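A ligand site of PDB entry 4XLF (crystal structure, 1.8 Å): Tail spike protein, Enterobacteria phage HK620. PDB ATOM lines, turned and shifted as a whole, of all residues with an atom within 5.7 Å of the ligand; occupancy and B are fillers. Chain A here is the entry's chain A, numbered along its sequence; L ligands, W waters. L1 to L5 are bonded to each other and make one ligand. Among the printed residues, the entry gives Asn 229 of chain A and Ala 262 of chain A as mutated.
O of Gly 101 touches O2 of LG5 L5, at 3.6 Å. CZ of Phe 137 touches C6 of LG5 L5, at 3.96 Å. CD1 of Leu 172 touches O5 of LG3 L3 (3.4 Å). CG2 of Thr 197 touches O5 of LG2 L2, at 3.4 Å. Thr 201 touches the ligand. O of Gly 203 touches O2 of LG4 L4, 3.98 Å away. NE1 of Trp 204 touches O1 of LG4 L4, 3.5 Å away. N of His 230 touches C8 of LIG L1, at 3.8 Å. N of Ser 231 touches C8 of LIG L1, 3.6 Å away. CG of Tyr 283 touches O4 of LIG L1 (3.1 Å). Val 285 touches the ligand. CB of Ala 289 touches C8 of LG4 L4 (3.96 Å). Within 4 Å of the ligand: Gly 101, His 102, Gln 132, Phe 137, Leu 172, Thr 197, Trp 198, Thr 201, Gly 203, Trp 204, Asn 205, Asn 229, His 230, Ser 231, Tyr 234, Asn 236, His 264, Tyr 283, Val 285, His 287, Ala 289, Glu 290 and Asn 361. The nearest printed residue that does not touch the ligand is Pro 142 (4.1 Å).
The side-chain hydroxyl (OH) of Tyr 234 sits close to a ring nitrogen (ND1) of His 264 (3.1 Å). N of Ser 231 sits at hydrogen-bond distance from O of Thr 197, at 2.9 Å. The backbone carbonyl oxygen (O) of His 102 sits at hydrogen-bond distance from the side-chain amide nitrogen (NE2) of Gln 132, 3.0 Å away. The backbone carbonyl oxygen of Thr 197 lies close to a ring nitrogen (ND1) of His 230 (3.3 Å). The backbone NH of Asn 236 lies within hydrogen-bond range of the backbone carbonyl oxygen of Leu 202, at 2.7 Å. The backbone carbonyl oxygen (O) of Ser 103 is in hydrogen-bond range of the backbone NH (N) of Gln 132 (2.9 Å). The backbone NH (N) of Asn 205 sits close to the side-chain amide nitrogen (ND2) of Asn 236 (3.1 Å). The backbone NH (N) of Leu 202 is in hydrogen-bond range of the backbone carbonyl oxygen (O) of Tyr 234, 2.9 Å away.
Water W10 lies within hydrogen-bond range of an oxygen (O2) of LG5 L5 (2.6 Å) and the backbone carbonyl oxygen (O) of Gly 101 (2.9 Å). Water W11 bridges an oxygen (O3) of LG5 L5 (2.6 Å) and the side-chain amide oxygen (OE1) of Gln 132 (2.7 Å). Water W9 bridges OG1 of Thr 201 (2.7 Å) and O4 of LG4 L4 (2.7 Å). Water W5 lies within hydrogen-bond range of O1 of LG2 L2 (2.9 Å) and ND2 of Asn 361 (3.5 Å). Water W6 lies within hydrogen-bond range of an oxygen (O1) of LG4 L4 (3.0 Å) and the indole nitrogen of Trp 204 (3.0 Å). Water W1 bridges the side-chain amide nitrogen of Asn 205 (3.0 Å) and an oxygen (O5) of LG4 L4 (3.0 Å).
The indole nitrogen of Trp 198 is in hydrogen-bond range of an oxygen (O5) of LIG L1. An oxygen (O3) of LG5 L5 is in hydrogen-bond range of a ring nitrogen (ND1) of His 102, at 2.7 Å. The side-chain amide oxygen of Asn 205 lies within hydrogen-bond range of an oxygen (O1) of LG4 L4 (2.7 Å). The side-chain carboxylate (OE2) of Glu 290 lies within hydrogen-bond range of a nitrogen (N1) of LG4 L4 (2.9 Å). A ring nitrogen (NE2) of His 264 sits at hydrogen-bond distance from an oxygen (O4) of LIG L1 (2.9 Å). The side-chain hydroxyl of Tyr 234 is in hydrogen-bond range of an oxygen (O1) of LG2 L2 (2.8 Å). The side-chain amide nitrogen of Asn 236 sits at hydrogen-bond distance from an oxygen (O2) of LG4 L4 (2.7 Å). A ring nitrogen (NE2) of His 287 is in hydrogen-bond range of an oxygen (O3) of LIG L1, at 2.6 Å. NE2 of Gln 132 lies within hydrogen-bond range of O3 of LG5 L5 (3.1 Å). An oxygen (O3) of LIG L1 sits at hydrogen-bond distance from the side-chain amide nitrogen of Asn 361. The side-chain amide nitrogen (ND2) of Asn 229 sits at hydrogen-bond distance from an oxygen (O6) of LIG L1 (3.1 Å).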
ATOM      1  N   GLY A 101      31.159  -3.435 -37.051  1.00  0.00           N
ATOM      2  CA  GLY A 101      31.020  -2.108 -36.454  1.00  0.00           C
ATOM      3  C   GLY A 101      30.646  -2.156 -34.969  1.00  0.00           C
ATOM      4  O   GLY A 101      30.710  -1.129 -34.286  1.00  0.00           O
ATOM      5  N   HIS A 102      30.253  -3.313 -34.461  1.00  0.00           N
ATOM      6  CA  HIS A 102      29.864  -3.493 -33.089  1.00  0.00           C
ATOM      7  C   HIS A 102      30.813  -4.430 -32.363  1.00  0.00           C
ATOM      8  O   HIS A 102      30.476  -4.936 -31.310  1.00  0.00           O
ATOM      9  CB  HIS A 102      28.466  -4.066 -33.022  1.00  0.00           C
ATOM     10  CG  HIS A 102      27.462  -3.318 -33.830  1.00  0.00           C
ATOM     11  ND1 HIS A 102      26.651  -2.362 -33.289  1.00  0.00           N
ATOM     12  CD2 HIS A 102      27.097  -3.440 -35.109  1.00  0.00           C
ATOM     13  CE1 HIS A 102      25.797  -1.932 -34.192  1.00  0.00           C
ATOM     14  NE2 HIS A 102      26.068  -2.554 -35.331  1.00  0.00           N
ATOM     15  N   SER A 103      32.027  -4.586 -32.904  1.00  0.00           N
ATOM     16  CA  SER A 103      33.012  -5.571 -32.312  1.00  0.00           C
ATOM     17  C   SER A 103      32.357  -6.924 -32.121  1.00  0.00           C
ATOM     18  O   SER A 103      32.695  -7.638 -31.201  1.00  0.00           O
ATOM     19  CB  SER A 103      33.570  -5.078 -31.005  1.00  0.00           C
ATOM     20  OG  SER A 103      33.985  -3.727 -31.137  1.00  0.00           O
ATOM     21  N   GLN A 132      31.341  -7.894 -28.614  1.00  0.00           N
ATOM     22  CA  GLN A 132      29.921  -8.111 -28.324  1.00  0.00           C
ATOM     23  C   GLN A 132      29.603  -9.424 -28.861  1.00  0.00           C
ATOM     24  O   GLN A 132      29.691  -9.664 -30.087  1.00  0.00           O
ATOM     25  CB  GLN A 132      29.069  -7.050 -28.967  1.00  0.00           C
ATOM     26  CG  GLN A 132      29.326  -5.669 -28.347  1.00  0.00           C
ATOM     27  CD  GLN A 132      28.248  -4.651 -28.724  1.00  0.00           C
ATOM     28  OE1 GLN A 132      27.034  -4.805 -28.419  1.00  0.00           O
ATOM     29  NE2 GLN A 132      28.687  -3.544 -29.279  1.00  0.00           N
ATOM     30  N   PHE A 137      22.124  -6.695 -34.859  1.00  0.00           N
ATOM     31  CA  PHE A 137      22.216  -5.705 -35.922  1.00  0.00           C
ATOM     32  C   PHE A 137      22.782  -6.379 -37.190  1.00  0.00           C
ATOM     33  O   PHE A 137      23.582  -7.294 -37.094  1.00  0.00           O
ATOM     34  CB  PHE A 137      23.131  -4.549 -35.503  1.00  0.00           C
ATOM     35  CG  PHE A 137      22.621  -3.700 -34.337  1.00  0.00           C
ATOM     36  CD1 PHE A 137      21.528  -2.843 -34.497  1.00  0.00           C
ATOM     37  CD2 PHE A 137      23.299  -3.703 -33.162  1.00  0.00           C
ATOM     38  CE1 PHE A 137      21.132  -2.045 -33.408  1.00  0.00           C
ATOM     39  CE2 PHE A 137      22.969  -2.906 -32.103  1.00  0.00           C
ATOM     40  CZ  PHE A 137      21.874  -2.056 -32.239  1.00  0.00           C
ATOM     41  N   PRO A 142      23.539   1.379 -36.620  1.00  0.00           N
ATOM     42  CA  PRO A 142      22.244   0.859 -36.169  1.00  0.00           C
ATOM     43  C   PRO A 142      21.059   1.522 -36.848  1.00  0.00           C
ATOM     44  O   PRO A 142      20.004   0.869 -37.091  1.00  0.00           O
ATOM     45  CB  PRO A 142      22.255   1.090 -34.650  1.00  0.00           C
ATOM     46  CG  PRO A 142      23.409   1.951 -34.339  1.00  0.00           C
ATOM     47  CD  PRO A 142      24.373   1.860 -35.511  1.00  0.00           C
ATOM     48  N   LEU A 172      33.840  -0.995 -25.267  1.00  0.00           N
ATOM     49  CA  LEU A 172      32.508  -1.582 -24.902  1.00  0.00           C
ATOM     50  C   LEU A 172      32.565  -3.118 -25.027  1.00  0.00           C
ATOM     51  O   LEU A 172      33.218  -3.701 -25.931  1.00  0.00           O
ATOM     52  CB  LEU A 172      31.349  -1.030 -25.774  1.00  0.00           C
ATOM     53  CG  LEU A 172      31.200   0.503 -25.847  1.00  0.00           C
ATOM     54  CD1 LEU A 172      30.362   0.968 -27.046  1.00  0.00           C
ATOM     55  CD2 LEU A 172      30.679   1.056 -24.563  1.00  0.00           C
ATOM     56  N   ASN A 174      29.772  -6.579 -24.450  1.00  0.00           N
ATOM     57  CA  ASN A 174      28.362  -7.018 -24.318  1.00  0.00           C
ATOM     58  C   ASN A 174      28.348  -8.533 -24.532  1.00  0.00           C
ATOM     59  O   ASN A 174      29.194  -9.063 -25.245  1.00  0.00           O
ATOM     60  CB  ASN A 174      27.491  -6.297 -25.363  1.00  0.00           C
ATOM     61  CG  ASN A 174      25.973  -6.369 -25.093  1.00  0.00           C
ATOM     62  OD1 ASN A 174      25.456  -6.870 -24.069  1.00  0.00           O
ATOM     63  ND2 ASN A 174      25.226  -5.758 -26.018  1.00  0.00           N
ATOM     64  N   THR A 197      30.446  -4.195 -20.196  1.00  0.00           N
ATOM     65  CA  THR A 197      29.695  -3.020 -20.039  1.00  0.00           C
ATOM     66  C   THR A 197      28.208  -3.426 -19.730  1.00  0.00           C
ATOM     67  O   THR A 197      27.535  -2.858 -18.850  1.00  0.00           O
ATOM     68  CB  THR A 197      29.695  -2.215 -21.335  1.00  0.00           C
ATOM     69  OG1 THR A 197      31.041  -1.942 -21.785  1.00  0.00           O
ATOM     70  CG2 THR A 197      28.902  -0.950 -21.109  1.00  0.00           C
ATOM     71  N   TRP A 198      27.736  -4.376 -20.492  1.00  0.00           N
ATOM     72  CA  TRP A 198      26.364  -4.985 -20.356  1.00  0.00           C
ATOM     73  C   TRP A 198      26.509  -6.505 -20.582  1.00  0.00           C
ATOM     74  O   TRP A 198      27.476  -6.953 -21.280  1.00  0.00           O
ATOM     75  CB  TRP A 198      25.401  -4.480 -21.410  1.00  0.00           C
ATOM     76  CG  TRP A 198      25.380  -3.050 -21.683  1.00  0.00           C
ATOM     77  CD1 TRP A 198      24.793  -2.087 -20.947  1.00  0.00           C
ATOM     78  CD2 TRP A 198      25.992  -2.401 -22.824  1.00  0.00           C
ATOM     79  NE1 TRP A 198      24.966  -0.859 -21.577  1.00  0.00           N
ATOM     80  CE2 TRP A 198      25.753  -1.029 -22.685  1.00  0.00           C
ATOM     81  CE3 TRP A 198      26.732  -2.866 -23.911  1.00  0.00           C
ATOM     82  CZ2 TRP A 198      26.230  -0.086 -23.635  1.00  0.00           C
ATOM     83  CZ3 TRP A 198      27.246  -1.946 -24.819  1.00  0.00           C
ATOM     84  CH2 TRP A 198      26.945  -0.572 -24.680  1.00  0.00           C
ATOM     85  N   THR A 201      21.603  -6.475 -24.064  1.00  0.00           N
ATOM     86  CA  THR A 201      20.829  -5.308 -24.395  1.00  0.00           C
ATOM     87  C   THR A 201      19.679  -5.602 -25.346  1.00  0.00           C
ATOM     88  O   THR A 201      19.798  -6.488 -26.205  1.00  0.00           O
ATOM     89  CB  THR A 201      21.669  -4.235 -25.095  1.00  0.00           C
ATOM     90  OG1 THR A 201      22.107  -4.698 -26.377  1.00  0.00           O
ATOM     91  CG2 THR A 201      22.839  -3.849 -24.220  1.00  0.00           C
ATOM     92  N   LEU A 202      18.571  -4.931 -25.103  1.00  0.00           N
ATOM     93  CA  LEU A 202      17.349  -5.208 -25.795  1.00  0.00           C
ATOM     94  C   LEU A 202      16.996  -3.940 -26.534  1.00  0.00           C
ATOM     95  O   LEU A 202      16.943  -2.854 -25.927  1.00  0.00           O
ATOM     96  CB  LEU A 202      16.220  -5.520 -24.837  1.00  0.00           C
ATOM     97  CG  LEU A 202      16.470  -6.599 -23.807  1.00  0.00           C
ATOM     98  CD1 LEU A 202      15.257  -6.758 -22.887  1.00  0.00           C
ATOM     99  CD2 LEU A 202      16.885  -7.915 -24.440  1.00  0.00           C
ATOM    100  N   GLY A 203      16.775  -4.076 -27.806  1.00  0.00           N
ATOM    101  CA  GLY A 203      16.277  -2.919 -28.589  1.00  0.00           C
ATOM    102  C   GLY A 203      17.358  -1.933 -28.919  1.00  0.00           C
ATOM    103  O   GLY A 203      18.505  -2.073 -28.508  1.00  0.00           O
ATOM    104  N   TRP A 204      16.976  -0.898 -29.651  1.00  0.00           N
ATOM    105  CA  TRP A 204      17.872   0.180 -30.048  1.00  0.00           C
ATOM    106  C   TRP A 204      17.080   1.448 -30.170  1.00  0.00           C
ATOM    107  O   TRP A 204      16.264   1.585 -31.092  1.00  0.00           O
ATOM    108  CB  TRP A 204      18.676  -0.097 -31.327  1.00  0.00           C
ATOM    109  CG  TRP A 204      19.543   1.059 -31.683  1.00  0.00           C
ATOM    110  CD1 TRP A 204      20.673   1.440 -31.041  1.00  0.00           C
ATOM    111  CD2 TRP A 204      19.262   2.054 -32.666  1.00  0.00           C
ATOM    112  NE1 TRP A 204      21.158   2.612 -31.584  1.00  0.00           N
ATOM    113  CE2 TRP A 204      20.318   3.017 -32.592  1.00  0.00           C
ATOM    114  CE3 TRP A 204      18.253   2.239 -33.608  1.00  0.00           C
ATOM    115  CZ2 TRP A 204      20.372   4.097 -33.414  1.00  0.00           C
ATOM    116  CZ3 TRP A 204      18.305   3.316 -34.443  1.00  0.00           C
ATOM    117  CH2 TRP A 204      19.370   4.253 -34.352  1.00  0.00           C
ATOM    118  N   ASN A 205      17.345   2.367 -29.241  1.00  0.00           N
ATOM    119  CA  ASN A 205      16.762   3.704 -29.212  1.00  0.00           C
ATOM    120  C   ASN A 205      15.294   3.725 -29.507  1.00  0.00           C
ATOM    121  O   ASN A 205      14.836   4.487 -30.334  1.00  0.00           O
ATOM    122  CB  ASN A 205      17.512   4.654 -30.118  1.00  0.00           C
ATOM    123  CG  ASN A 205      18.904   4.965 -29.648  1.00  0.00           C
ATOM    124  OD1 ASN A 205      19.366   4.482 -28.595  1.00  0.00           O
ATOM    125  ND2 ASN A 205      19.633   5.712 -30.480  1.00  0.00           N
ATOM    126  N   ASN A 229      31.805   1.650 -16.549  1.00  0.00           N
ATOM    127  CA  ASN A 229      30.349   1.710 -16.317  1.00  0.00           C
ATOM    128  C   ASN A 229      29.786   0.402 -16.695  1.00  0.00           C
ATOM    129  O   ASN A 229      30.244  -0.226 -17.676  1.00  0.00           O
ATOM    130  CB  ASN A 229      29.733   2.816 -17.177  1.00  0.00           C
ATOM    131  CG  ASN A 229      28.413   3.336 -16.651  1.00  0.00           C
ATOM    132  OD1 ASN A 229      27.659   2.666 -15.916  1.00  0.00           O
ATOM    133  ND2 ASN A 229      28.103   4.542 -17.067  1.00  0.00           N
ATOM    134  N   HIS A 230      28.804  -0.034 -15.922  1.00  0.00           N
ATOM    135  CA  HIS A 230      28.158  -1.302 -16.181  1.00  0.00           C
ATOM    136  C   HIS A 230      26.686  -1.294 -15.851  1.00  0.00           C
ATOM    137  O   HIS A 230      26.336  -0.768 -14.800  1.00  0.00           O
ATOM    138  CB  HIS A 230      28.803  -2.391 -15.356  1.00  0.00           C
ATOM    139  CG  HIS A 230      28.134  -3.732 -15.498  1.00  0.00           C
ATOM    140  ND1 HIS A 230      28.624  -4.741 -16.309  1.00  0.00           N
ATOM    141  CD2 HIS A 230      27.045  -4.245 -14.879  1.00  0.00           C
ATOM    142  CE1 HIS A 230      27.858  -5.799 -16.185  1.00  0.00           C
ATOM    143  NE2 HIS A 230      26.899  -5.527 -15.320  1.00  0.00           N
ATOM    144  N   SER A 231      25.881  -1.790 -16.773  1.00  0.00           N
ATOM    145  CA  SER A 231      24.428  -2.064 -16.577  1.00  0.00           C
ATOM    146  C   SER A 231      24.149  -3.464 -17.140  1.00  0.00           C
ATOM    147  O   SER A 231      24.300  -3.691 -18.319  1.00  0.00           O
ATOM    148  CB  SER A 231      23.523  -1.040 -17.236  1.00  0.00           C
ATOM    149  OG  SER A 231      22.189  -1.321 -16.866  1.00  0.00           O
ATOM    150  N   TYR A 234      20.262  -3.701 -20.383  1.00  0.00           N
ATOM    151  CA  TYR A 234      19.743  -2.424 -20.822  1.00  0.00           C
ATOM    152  C   TYR A 234      18.505  -2.603 -21.724  1.00  0.00           C
ATOM    153  O   TYR A 234      18.585  -3.266 -22.754  1.00  0.00           O
ATOM    154  CB  TYR A 234      20.861  -1.671 -21.536  1.00  0.00           C
ATOM    155  CG  TYR A 234      20.816  -0.161 -21.690  1.00  0.00           C
ATOM    156  CD1 TYR A 234      19.939   0.461 -22.565  1.00  0.00           C
ATOM    157  CD2 TYR A 234      21.743   0.648 -21.039  1.00  0.00           C
ATOM    158  CE1 TYR A 234      19.950   1.863 -22.729  1.00  0.00           C
ATOM    159  CE2 TYR A 234      21.742   2.022 -21.226  1.00  0.00           C
ATOM    160  CZ  TYR A 234      20.880   2.631 -22.078  1.00  0.00           C
ATOM    161  OH  TYR A 234      20.944   4.002 -22.308  1.00  0.00           O
ATOM    162  N   ASN A 236      16.003  -1.079 -24.081  1.00  0.00           N
ATOM    163  CA  ASN A 236      15.875   0.081 -24.938  1.00  0.00           C
ATOM    164  C   ASN A 236      14.820  -0.112 -26.033  1.00  0.00           C
ATOM    165  O   ASN A 236      14.895   0.457 -27.095  1.00  0.00           O
ATOM    166  CB  ASN A 236      17.226   0.419 -25.551  1.00  0.00           C
ATOM    167  CG  ASN A 236      17.403   1.923 -25.811  1.00  0.00           C
ATOM    168  OD1 ASN A 236      16.518   2.701 -25.562  1.00  0.00           O
ATOM    169  ND2 ASN A 236      18.564   2.277 -26.360  1.00  0.00           N
ATOM    170  N   ALA A 262      18.662  -1.199 -16.637  1.00  0.00           N
ATOM    171  CA  ALA A 262      18.249   0.108 -17.058  1.00  0.00           C
ATOM    172  C   ALA A 262      16.915  -0.052 -17.807  1.00  0.00           C
ATOM    173  O   ALA A 262      16.875  -0.720 -18.843  1.00  0.00           O
ATOM    174  CB  ALA A 262      19.267   0.749 -17.994  1.00  0.00           C
ATOM    175  N   HIS A 264      14.524   1.951 -20.123  1.00  0.00           N
ATOM    176  CA  HIS A 264      14.640   3.191 -20.857  1.00  0.00           C
ATOM    177  C   HIS A 264      13.590   3.465 -21.933  1.00  0.00           C
ATOM    178  O   HIS A 264      13.767   4.399 -22.737  1.00  0.00           O
ATOM    179  CB  HIS A 264      16.046   3.283 -21.500  1.00  0.00           C
ATOM    180  CG  HIS A 264      17.137   3.780 -20.599  1.00  0.00           C
ATOM    181  ND1 HIS A 264      18.185   4.515 -21.092  1.00  0.00           N
ATOM    182  CD2 HIS A 264      17.369   3.654 -19.283  1.00  0.00           C
ATOM    183  CE1 HIS A 264      19.025   4.826 -20.120  1.00  0.00           C
ATOM    184  NE2 HIS A 264      18.596   4.253 -19.023  1.00  0.00           N
ATOM    185  N   TYR A 283      18.103   1.849 -13.163  1.00  0.00           N
ATOM    186  CA  TYR A 283      17.766   3.167 -13.747  1.00  0.00           C
ATOM    187  C   TYR A 283      16.367   3.104 -14.447  1.00  0.00           C
ATOM    188  O   TYR A 283      16.061   2.176 -15.168  1.00  0.00           O
ATOM    189  CB  TYR A 283      18.808   3.662 -14.776  1.00  0.00           C
ATOM    190  CG  TYR A 283      20.100   4.091 -14.141  1.00  0.00           C
ATOM    191  CD1 TYR A 283      20.264   5.403 -13.693  1.00  0.00           C
ATOM    192  CD2 TYR A 283      21.173   3.213 -13.968  1.00  0.00           C
ATOM    193  CE1 TYR A 283      21.455   5.820 -13.108  1.00  0.00           C
ATOM    194  CE2 TYR A 283      22.328   3.637 -13.409  1.00  0.00           C
ATOM    195  CZ  TYR A 283      22.477   4.929 -12.978  1.00  0.00           C
ATOM    196  OH  TYR A 283      23.656   5.313 -12.379  1.00  0.00           O
ATOM    197  N   VAL A 285      14.659   5.822 -16.847  1.00  0.00           N
ATOM    198  CA  VAL A 285      15.152   7.083 -17.421  1.00  0.00           C
ATOM    199  C   VAL A 285      14.601   7.185 -18.817  1.00  0.00           C
ATOM    200  O   VAL A 285      14.546   6.168 -19.538  1.00  0.00           O
ATOM    201  CB  VAL A 285      16.692   7.081 -17.442  1.00  0.00           C
ATOM    202  CG1 VAL A 285      17.244   8.330 -18.210  1.00  0.00           C
ATOM    203  CG2 VAL A 285      17.265   7.065 -16.021  1.00  0.00           C
ATOM    204  N   HIS A 287      16.028   9.058 -21.902  1.00  0.00           N
ATOM    205  CA  HIS A 287      17.025   9.867 -22.611  1.00  0.00           C
ATOM    206  C   HIS A 287      16.427  10.405 -23.932  1.00  0.00           C
ATOM    207  O   HIS A 287      15.995   9.607 -24.826  1.00  0.00           O
ATOM    208  CB  HIS A 287      18.225   9.041 -22.998  1.00  0.00           C
ATOM    209  CG  HIS A 287      19.170   8.717 -21.886  1.00  0.00           C
ATOM    210  ND1 HIS A 287      19.500   9.568 -20.867  1.00  0.00           N
ATOM    211  CD2 HIS A 287      19.913   7.595 -21.668  1.00  0.00           C
ATOM    212  CE1 HIS A 287      20.382   9.003 -20.067  1.00  0.00           C
ATOM    213  NE2 HIS A 287      20.606   7.774 -20.497  1.00  0.00           N
ATOM    214  N   ALA A 289      18.049  11.410 -26.262  1.00  0.00           N
ATOM    215  CA  ALA A 289      18.868  10.774 -27.278  1.00  0.00           C
ATOM    216  C   ALA A 289      18.440   9.411 -27.750  1.00  0.00           C
ATOM    217  O   ALA A 289      18.978   8.913 -28.756  1.00  0.00           O
ATOM    218  CB  ALA A 289      20.314  10.681 -26.759  1.00  0.00           C
ATOM    219  N   GLU A 290      17.547   8.751 -27.014  1.00  0.00           N
ATOM    220  CA  GLU A 290      17.123   7.440 -27.321  1.00  0.00           C
ATOM    221  C   GLU A 290      15.662   7.419 -27.754  1.00  0.00           C
ATOM    222  O   GLU A 290      15.054   6.386 -27.768  1.00  0.00           O
ATOM    223  CB  GLU A 290      17.340   6.528 -26.070  1.00  0.00           C
ATOM    224  CG  GLU A 290      18.816   6.424 -25.712  1.00  0.00           C
ATOM    225  CD  GLU A 290      19.082   5.495 -24.558  1.00  0.00           C
ATOM    226  OE1 GLU A 290      18.184   5.338 -23.691  1.00  0.00           O
ATOM    227  OE2 GLU A 290      20.178   4.939 -24.480  1.00  0.00           O
ATOM    228  N   ASN A 361      23.366  13.124 -17.428  1.00  0.00           N
ATOM    229  CA  ASN A 361      24.749  12.669 -17.511  1.00  0.00           C
ATOM    230  C   ASN A 361      25.791  13.794 -17.514  1.00  0.00           C
ATOM    231  O   ASN A 361      26.899  13.545 -17.158  1.00  0.00           O
ATOM    232  CB  ASN A 361      24.986  11.720 -18.713  1.00  0.00           C
ATOM    233  CG  ASN A 361      24.350  10.365 -18.495  1.00  0.00           C
ATOM    234  OD1 ASN A 361      23.950  10.052 -17.388  1.00  0.00           O
ATOM    235  ND2 ASN A 361      24.240   9.555 -19.549  1.00  0.00           N
HETATM  236  C1  LIG L   1      23.983   4.122 -16.730  1.00  0.00           C
HETATM  237  C2  LIG L   1      24.159   3.731 -18.202  1.00  0.00           C
HETATM  238  C3  LIG L   1      24.215   4.996 -19.070  1.00  0.00           C
HETATM  239  C4  LIG L   1      22.919   5.816 -18.801  1.00  0.00           C
HETATM  240  C5  LIG L   1      22.649   6.089 -17.276  1.00  0.00           C
HETATM  241  C6  LIG L   1      21.171   6.530 -17.019  1.00  0.00           C
HETATM  242  C7  LIG L   1      25.403   1.784 -19.022  1.00  0.00           C
HETATM  243  C8  LIG L   1      26.661   1.006 -18.919  1.00  0.00           C
HETATM  244  O1  LIG L   1      22.827   4.894 -16.513  1.00  0.00           O
HETATM  245  O2  LIG L   1      24.326   4.679 -20.467  1.00  0.00           O
HETATM  246  O3  LIG L   1      22.896   7.061 -19.497  1.00  0.00           O
HETATM  247  O4  LIG L   1      20.406   5.245 -17.051  1.00  0.00           O
HETATM  248  O5  LIG L   1      24.473   1.440 -19.796  1.00  0.00           O
HETATM  249  N1  LIG L   1      25.340   2.888 -18.251  1.00  0.00           N
HETATM  250  O6  LIG L   1      25.100   4.832 -16.317  1.00  0.00           O
HETATM  251  C1  LG2 L   2      25.080   5.647 -21.203  1.00  0.00           C
HETATM  252  C2  LG2 L   2      24.594   5.481 -22.648  1.00  0.00           C
HETATM  253  C3  LG2 L   2      24.942   4.061 -23.182  1.00  0.00           C
HETATM  254  C4  LG2 L   2      26.405   3.739 -22.965  1.00  0.00           C
HETATM  255  C5  LG2 L   2      26.749   3.933 -21.480  1.00  0.00           C
HETATM  256  C6  LG2 L   2      28.208   3.723 -21.123  1.00  0.00           C
HETATM  257  O1  LG2 L   2      23.184   5.676 -22.683  1.00  0.00           O
HETATM  258  O2  LG2 L   2      24.615   4.066 -24.567  1.00  0.00           O
HETATM  259  O3  LG2 L   2      27.238   4.644 -23.751  1.00  0.00           O
HETATM  260  O4  LG2 L   2      26.423   5.288 -21.081  1.00  0.00           O
HETATM  261  O5  LG2 L   2      28.642   2.423 -21.530  1.00  0.00           O
HETATM  262  C1  LG3 L   3      28.231   3.943 -24.517  1.00  0.00           C
HETATM  263  C2  LG3 L   3      29.195   4.971 -25.123  1.00  0.00           C
HETATM  264  C3  LG3 L   3      28.503   5.834 -26.206  1.00  0.00           C
HETATM  265  C4  LG3 L   3      27.973   4.888 -27.250  1.00  0.00           C
HETATM  266  C5  LG3 L   3      26.964   3.913 -26.583  1.00  0.00           C
HETATM  267  C6  LG3 L   3      26.329   2.873 -27.512  1.00  0.00           C
HETATM  268  O1  LG3 L   3      29.655   5.817 -24.082  1.00  0.00           O
HETATM  269  O2  LG3 L   3      29.531   6.653 -26.755  1.00  0.00           O
HETATM  270  O3  LG3 L   3      27.336   5.644 -28.236  1.00  0.00           O
HETATM  271  O4  LG3 L   3      27.676   3.169 -25.559  1.00  0.00           O
HETATM  272  O5  LG3 L   3      27.412   2.149 -28.162  1.00  0.00           O
HETATM  273  C1  LG4 L   4      23.437   3.282 -24.866  1.00  0.00           C
HETATM  274  C2  LG4 L   4      22.990   3.832 -26.236  1.00  0.00           C
HETATM  275  C3  LG4 L   4      21.850   2.990 -26.798  1.00  0.00           C
HETATM  276  C4  LG4 L   4      22.027   1.483 -26.646  1.00  0.00           C
HETATM  277  C5  LG4 L   4      22.453   1.195 -25.260  1.00  0.00           C
HETATM  278  C6  LG4 L   4      22.808  -0.230 -25.050  1.00  0.00           C
HETATM  279  C7  LG4 L   4      23.181   6.227 -26.564  1.00  0.00           C
HETATM  280  C8  LG4 L   4      22.716   7.591 -26.165  1.00  0.00           C
HETATM  281  N1  LG4 L   4      22.600   5.199 -25.977  1.00  0.00           N
HETATM  282  O1  LG4 L   4      21.720   3.334 -28.164  1.00  0.00           O
HETATM  283  O2  LG4 L   4      20.768   0.792 -26.929  1.00  0.00           O
HETATM  284  O3  LG4 L   4      23.630   1.883 -24.966  1.00  0.00           O
HETATM  285  O4  LG4 L   4      23.836  -0.693 -25.891  1.00  0.00           O
HETATM  286  O5  LG4 L   4      24.050   6.091 -27.435  1.00  0.00           O
HETATM  287  C1  LG5 L   5      27.331   2.419 -29.579  1.00  0.00           C
HETATM  288  C2  LG5 L   5      28.502   1.678 -30.216  1.00  0.00           C
HETATM  289  C3  LG5 L   5      28.262   0.209 -30.229  1.00  0.00           C
HETATM  290  C4  LG5 L   5      26.880  -0.129 -30.790  1.00  0.00           C
HETATM  291  C5  LG5 L   5      25.845   0.623 -30.006  1.00  0.00           C
HETATM  292  C6  LG5 L   5      24.443   0.496 -30.637  1.00  0.00           C
HETATM  293  O1  LG5 L   5      28.618   2.155 -31.562  1.00  0.00           O
HETATM  294  O2  LG5 L   5      29.288  -0.334 -31.092  1.00  0.00           O
HETATM  295  O3  LG5 L   5      26.731  -1.564 -30.734  1.00  0.00           O
HETATM  296  O4  LG5 L   5      26.098   2.036 -30.143  1.00  0.00           O
HETATM  297  O   HOH W   1      22.469   6.414 -29.965  1.00  0.00           O
HETATM  298  O   HOH W   2      19.686  -1.669 -25.252  1.00  0.00           O
HETATM  299  O   HOH W   3      31.104   2.120 -20.679  1.00  0.00           O
HETATM  300  O   HOH W   4      28.018   7.270 -22.420  1.00  0.00           O
HETATM  301  O   HOH W   5      23.258   8.557 -22.726  1.00  0.00           O
HETATM  302  O   HOH W   6      23.598   3.828 -30.400  1.00  0.00           O
HETATM  303  O   HOH W   7      21.064  -1.056 -28.771  1.00  0.00           O
HETATM  304  O   HOH W   8      25.878   5.026 -13.807  1.00  0.00           O
HETATM  305  O   HOH W   9      23.204  -2.657 -27.708  1.00  0.00           O
HETATM  306  O   HOH W  10      31.538   0.506 -32.075  1.00  0.00           O
HETATM  307  O   HOH W  11      25.150  -3.195 -29.399  1.00  0.00           O
HETATM  308  O   HOH W  12      32.496   4.657 -24.561  1.00  0.00           O
HETATM  309  O   HOH W  13      28.916   8.959 -28.328  1.00  0.00           O
HETATM  310  O   HOH W  14      31.075   8.253 -25.427  1.00  0.00           O
HETATM  311  O   HOH W  15      31.955   6.260 -27.561  1.00  0.00           O
HETATM  312  O   HOH W  16      31.628  -1.856 -29.785  1.00  0.00           O
